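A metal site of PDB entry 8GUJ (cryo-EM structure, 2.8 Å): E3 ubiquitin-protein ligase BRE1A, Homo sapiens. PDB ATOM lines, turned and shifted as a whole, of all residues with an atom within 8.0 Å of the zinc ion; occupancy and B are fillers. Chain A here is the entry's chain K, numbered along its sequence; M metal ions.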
ATOM      1  N   LEU A 934      -9.243 -26.862  -3.019  1.00  0.00           N
ATOM      2  CA  LEU A 934     -10.487 -27.230  -2.358  1.00  0.00           C
ATOM      3  C   LEU A 934     -11.593 -26.313  -2.878  1.00  0.00           C
ATOM      4  O   LEU A 934     -11.524 -25.090  -2.686  1.00  0.00           O
ATOM      5  CB  LEU A 934     -10.358 -27.112  -0.841  1.00  0.00           C
ATOM      6  CG  LEU A 934      -9.147 -27.752  -0.164  1.00  0.00           C
ATOM      7  CD1 LEU A 934      -9.245 -27.596   1.348  1.00  0.00           C
ATOM      8  CD2 LEU A 934      -9.018 -29.215  -0.546  1.00  0.00           C
ATOM      9  N   THR A 935     -12.592 -26.892  -3.536  1.00  0.00           N
ATOM     10  CA  THR A 935     -13.557 -26.067  -4.262  1.00  0.00           C
ATOM     11  C   THR A 935     -14.681 -25.560  -3.358  1.00  0.00           C
ATOM     12  O   THR A 935     -15.426 -24.653  -3.750  1.00  0.00           O
ATOM     13  CB  THR A 935     -14.124 -26.850  -5.447  1.00  0.00           C
ATOM     14  OG1 THR A 935     -14.586 -28.123  -5.007  1.00  0.00           O
ATOM     15  CG2 THR A 935     -13.063 -27.047  -6.515  1.00  0.00           C
ATOM     16  N   LYS A 936     -14.837 -26.141  -2.168  1.00  0.00           N
ATOM     17  CA  LYS A 936     -15.797 -25.588  -1.211  1.00  0.00           C
ATOM     18  C   LYS A 936     -15.296 -24.280  -0.620  1.00  0.00           C
ATOM     19  O   LYS A 936     -16.010 -23.277  -0.592  1.00  0.00           O
ATOM     20  CB  LYS A 936     -16.102 -26.601  -0.115  1.00  0.00           C
ATOM     21  CG  LYS A 936     -17.558 -27.059  -0.091  1.00  0.00           C
ATOM     22  CD  LYS A 936     -17.961 -27.790  -1.362  1.00  0.00           C
ATOM     23  CE  LYS A 936     -19.406 -28.243  -1.288  1.00  0.00           C
ATOM     24  NZ  LYS A 936     -19.902 -28.765  -2.594  1.00  0.00           N
ATOM     25  N   CYS A 937     -14.047 -24.260  -0.143  1.00  0.00           N
ATOM     26  CA  CYS A 937     -13.506 -23.069   0.485  1.00  0.00           C
ATOM     27  C   CYS A 937     -12.720 -22.188  -0.468  1.00  0.00           C
ATOM     28  O   CYS A 937     -12.223 -21.136  -0.045  1.00  0.00           O
ATOM     29  CB  CYS A 937     -12.620 -23.454   1.680  1.00  0.00           C
ATOM     30  SG  CYS A 937     -11.128 -24.368   1.267  1.00  0.00           S
ATOM     31  N   PHE A 938     -12.601 -22.584  -1.743  1.00  0.00           N
ATOM     32  CA  PHE A 938     -11.895 -21.803  -2.765  1.00  0.00           C
ATOM     33  C   PHE A 938     -10.460 -21.499  -2.369  1.00  0.00           C
ATOM     34  O   PHE A 938      -9.951 -20.392  -2.565  1.00  0.00           O
ATOM     35  CB  PHE A 938     -12.655 -20.511  -3.085  1.00  0.00           C
ATOM     36  CG  PHE A 938     -13.780 -20.682  -4.075  1.00  0.00           C
ATOM     37  CD1 PHE A 938     -14.095 -21.943  -4.572  1.00  0.00           C
ATOM     38  CD2 PHE A 938     -14.529 -19.594  -4.495  1.00  0.00           C
ATOM     39  CE1 PHE A 938     -15.128 -22.104  -5.474  1.00  0.00           C
ATOM     40  CE2 PHE A 938     -15.562 -19.754  -5.397  1.00  0.00           C
ATOM     41  CZ  PHE A 938     -15.867 -21.013  -5.885  1.00  0.00           C
ATOM     42  N   HIS A 939      -9.793 -22.497  -1.796  1.00  0.00           N
ATOM     43  CA  HIS A 939      -8.414 -22.371  -1.348  1.00  0.00           C
ATOM     44  C   HIS A 939      -7.535 -23.399  -2.038  1.00  0.00           C
ATOM     45  O   HIS A 939      -8.009 -24.409  -2.582  1.00  0.00           O
ATOM     46  CB  HIS A 939      -8.309 -22.525   0.176  1.00  0.00           C
ATOM     47  CG  HIS A 939      -9.142 -21.551   0.935  1.00  0.00           C
ATOM     48  ND1 HIS A 939      -9.807 -21.875   2.100  1.00  0.00           N
ATOM     49  CD2 HIS A 939      -9.408 -20.239   0.708  1.00  0.00           C
ATOM     50  CE1 HIS A 939     -10.454 -20.820   2.551  1.00  0.00           C
ATOM     51  NE2 HIS A 939     -10.228 -19.806   1.721  1.00  0.00           N
ATOM     52  N   VAL A 940      -6.226 -23.135  -2.014  1.00  0.00           N
ATOM     53  CA  VAL A 940      -5.237 -23.934  -2.720  1.00  0.00           C
ATOM     54  C   VAL A 940      -4.246 -24.485  -1.707  1.00  0.00           C
ATOM     55  O   VAL A 940      -3.683 -23.727  -0.914  1.00  0.00           O
ATOM     56  CB  VAL A 940      -4.516 -23.098  -3.794  1.00  0.00           C
ATOM     57  CG1 VAL A 940      -3.406 -23.902  -4.451  1.00  0.00           C
ATOM     58  CG2 VAL A 940      -5.502 -22.609  -4.829  1.00  0.00           C
ATOM     59  N   PHE A 941      -4.063 -25.809  -1.726  1.00  0.00           N
ATOM     60  CA  PHE A 941      -3.037 -26.506  -0.950  1.00  0.00           C
ATOM     61  C   PHE A 941      -2.138 -27.295  -1.900  1.00  0.00           C
ATOM     62  O   PHE A 941      -2.231 -27.145  -3.117  1.00  0.00           O
ATOM     63  CB  PHE A 941      -3.649 -27.472   0.079  1.00  0.00           C
ATOM     64  CG  PHE A 941      -4.186 -26.807   1.321  1.00  0.00           C
ATOM     65  CD1 PHE A 941      -4.540 -27.584   2.414  1.00  0.00           C
ATOM     66  CD2 PHE A 941      -4.314 -25.437   1.428  1.00  0.00           C
ATOM     67  CE1 PHE A 941      -5.025 -27.006   3.567  1.00  0.00           C
ATOM     68  CE2 PHE A 941      -4.798 -24.850   2.578  1.00  0.00           C
ATOM     69  CZ  PHE A 941      -5.154 -25.636   3.643  1.00  0.00           C
ATOM     70  N   ARG A 949      -3.701 -36.021   4.740  1.00  0.00           N
ATOM     71  CA  ARG A 949      -4.614 -35.507   5.750  1.00  0.00           C
ATOM     72  C   ARG A 949      -6.050 -35.948   5.452  1.00  0.00           C
ATOM     73  O   ARG A 949      -6.915 -35.905   6.332  1.00  0.00           O
ATOM     74  CB  ARG A 949      -4.478 -33.982   5.818  1.00  0.00           C
ATOM     75  CG  ARG A 949      -5.142 -33.274   6.997  1.00  0.00           C
ATOM     76  CD  ARG A 949      -6.550 -32.829   6.698  1.00  0.00           C
ATOM     77  NE  ARG A 949      -6.602 -31.883   5.594  1.00  0.00           N
ATOM     78  CZ  ARG A 949      -7.702 -31.570   4.948  1.00  0.00           C
ATOM     79  NH1 ARG A 949      -8.870 -32.085   5.287  1.00  0.00           N
ATOM     80  NH2 ARG A 949      -7.641 -30.710   3.932  1.00  0.00           N
ATOM     81  N   LYS A 956     -11.775 -31.879   6.912  1.00  0.00           N
ATOM     82  CA  LYS A 956     -11.988 -30.456   7.184  1.00  0.00           C
ATOM     83  C   LYS A 956     -10.767 -29.680   6.724  1.00  0.00           C
ATOM     84  O   LYS A 956      -9.635 -30.164   6.804  1.00  0.00           O
ATOM     85  CB  LYS A 956     -12.239 -30.197   8.678  1.00  0.00           C
ATOM     86  CG  LYS A 956     -13.472 -30.887   9.235  1.00  0.00           C
ATOM     87  CD  LYS A 956     -14.737 -30.395   8.546  1.00  0.00           C
ATOM     88  CE  LYS A 956     -15.017 -28.938   8.872  1.00  0.00           C
ATOM     89  NZ  LYS A 956     -15.303 -28.736  10.312  1.00  0.00           N
ATOM     90  N   CYS A 957     -11.002 -28.453   6.250  1.00  0.00           N
ATOM     91  CA  CYS A 957      -9.896 -27.612   5.827  1.00  0.00           C
ATOM     92  C   CYS A 957      -9.116 -27.153   7.049  1.00  0.00           C
ATOM     93  O   CYS A 957      -9.722 -26.688   8.023  1.00  0.00           O
ATOM     94  CB  CYS A 957     -10.386 -26.411   5.022  1.00  0.00           C
ATOM     95  SG  CYS A 957      -9.037 -25.423   4.309  1.00  0.00           S
ATOM     96  N   PRO A 958      -7.792 -27.286   7.058  1.00  0.00           N
ATOM     97  CA  PRO A 958      -7.018 -26.890   8.249  1.00  0.00           C
ATOM     98  C   PRO A 958      -7.158 -25.436   8.634  1.00  0.00           C
ATOM     99  O   PRO A 958      -7.053 -25.117   9.832  1.00  0.00           O
ATOM    100  CB  PRO A 958      -5.574 -27.228   7.836  1.00  0.00           C
ATOM    101  CG  PRO A 958      -5.720 -28.363   6.880  1.00  0.00           C
ATOM    102  CD  PRO A 958      -7.008 -28.128   6.140  1.00  0.00           C
ATOM    103  N   LYS A 959      -7.383 -24.528   7.686  1.00  0.00           N
ATOM    104  CA  LYS A 959      -7.345 -23.096   7.988  1.00  0.00           C
ATOM    105  C   LYS A 959      -8.722 -22.443   8.030  1.00  0.00           C
ATOM    106  O   LYS A 959      -8.939 -21.547   8.846  1.00  0.00           O
ATOM    107  CB  LYS A 959      -6.432 -22.366   6.996  1.00  0.00           C
ATOM    108  CG  LYS A 959      -6.933 -22.272   5.569  1.00  0.00           C
ATOM    109  CD  LYS A 959      -5.874 -21.602   4.687  1.00  0.00           C
ATOM    110  CE  LYS A 959      -6.383 -21.374   3.280  1.00  0.00           C
ATOM    111  NZ  LYS A 959      -7.391 -20.285   3.237  1.00  0.00           N
ATOM    112  N   CYS A 960      -9.658 -22.866   7.191  1.00  0.00           N
ATOM    113  CA  CYS A 960     -10.989 -22.262   7.194  1.00  0.00           C
ATOM    114  C   CYS A 960     -12.075 -23.216   7.698  1.00  0.00           C
ATOM    115  O   CYS A 960     -13.233 -22.802   7.779  1.00  0.00           O
ATOM    116  CB  CYS A 960     -11.364 -21.767   5.798  1.00  0.00           C
ATOM    117  SG  CYS A 960     -11.816 -23.052   4.629  1.00  0.00           S
ATOM    118  N   ASN A 961     -11.712 -24.460   8.025  1.00  0.00           N
ATOM    119  CA  ASN A 961     -12.650 -25.437   8.594  1.00  0.00           C
ATOM    120  C   ASN A 961     -13.833 -25.708   7.671  1.00  0.00           C
ATOM    121  O   ASN A 961     -14.995 -25.588   8.072  1.00  0.00           O
ATOM    122  CB  ASN A 961     -13.126 -25.012   9.988  1.00  0.00           C
ATOM    123  CG  ASN A 961     -12.233 -25.531  11.100  1.00  0.00           C
ATOM    124  OD1 ASN A 961     -11.025 -25.712  10.907  1.00  0.00           O
ATOM    125  ND2 ASN A 961     -12.810 -25.767  12.263  1.00  0.00           N
ATOM    126  N   ALA A 962     -13.550 -26.064   6.430  1.00  0.00           N
ATOM    127  CA  ALA A 962     -14.578 -26.390   5.446  1.00  0.00           C
ATOM    128  C   ALA A 962     -14.581 -27.879   5.172  1.00  0.00           C
ATOM    129  O   ALA A 962     -13.541 -28.473   4.870  1.00  0.00           O
ATOM    130  CB  ALA A 962     -14.355 -25.605   4.154  1.00  0.00           C
ATOM    131  N   ALA A 963     -15.760 -28.492   5.280  1.00  0.00           N
ATOM    132  CA  ALA A 963     -15.897 -29.915   5.010  1.00  0.00           C
ATOM    133  C   ALA A 963     -15.978 -30.170   3.505  1.00  0.00           C
ATOM    134  O   ALA A 963     -16.660 -29.434   2.778  1.00  0.00           O
ATOM    135  CB  ALA A 963     -17.148 -30.473   5.703  1.00  0.00           C
ATOM    136  N   PHE A 964     -15.279 -31.201   3.044  1.00  0.00           N
ATOM    137  CA  PHE A 964     -15.257 -31.541   1.627  1.00  0.00           C
ATOM    138  C   PHE A 964     -15.221 -33.052   1.454  1.00  0.00           C
ATOM    139  O   PHE A 964     -14.790 -33.785   2.347  1.00  0.00           O
ATOM    140  CB  PHE A 964     -14.059 -30.902   0.909  1.00  0.00           C
ATOM    141  CG  PHE A 964     -12.726 -31.299   1.458  1.00  0.00           C
ATOM    142  CD1 PHE A 964     -12.065 -32.419   0.975  1.00  0.00           C
ATOM    143  CD2 PHE A 964     -12.122 -30.549   2.463  1.00  0.00           C
ATOM    144  CE1 PHE A 964     -10.840 -32.788   1.487  1.00  0.00           C
ATOM    145  CE2 PHE A 964     -10.897 -30.920   2.966  1.00  0.00           C
ATOM    146  CZ  PHE A 964     -10.257 -32.041   2.473  1.00  0.00           C
HETATM  147 ZN    ZN M   1     -10.069 -23.647   3.216  1.00  0.00          ZN
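A ring nitrogen (NE2) of His 939 lies close to the side-chain amino group of Lys 959 (3.3 Å).
The backbone NH (N) of Leu 934 lies within hydrogen-bond range of the backbone carbonyl oxygen (O) of His 939, at 2.8 Å.
N of Cys 957 lies within hydrogen-bond range of O of Ala 962, at 2.9 Å.
The backbone carbonyl oxygen (O) of Cys 957 lies close to the side-chain amide oxygen (OD1) of Asn 961, at 3.3 Å.
Within 4 Å of the zinc ion: Cys 937, His 939, Cys 957 and Cys 960.
The zinc ion is bound by a ring nitrogen (ND1) of His 939 (2.1 Å), the side-chain sulfur (SG) of Cys 960 (2.3 Å), the side-chain sulfur (SG) of Cys 957 (2.3 Å) and the side-chain sulfur (SG) of Cys 937 (2.3 Å).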
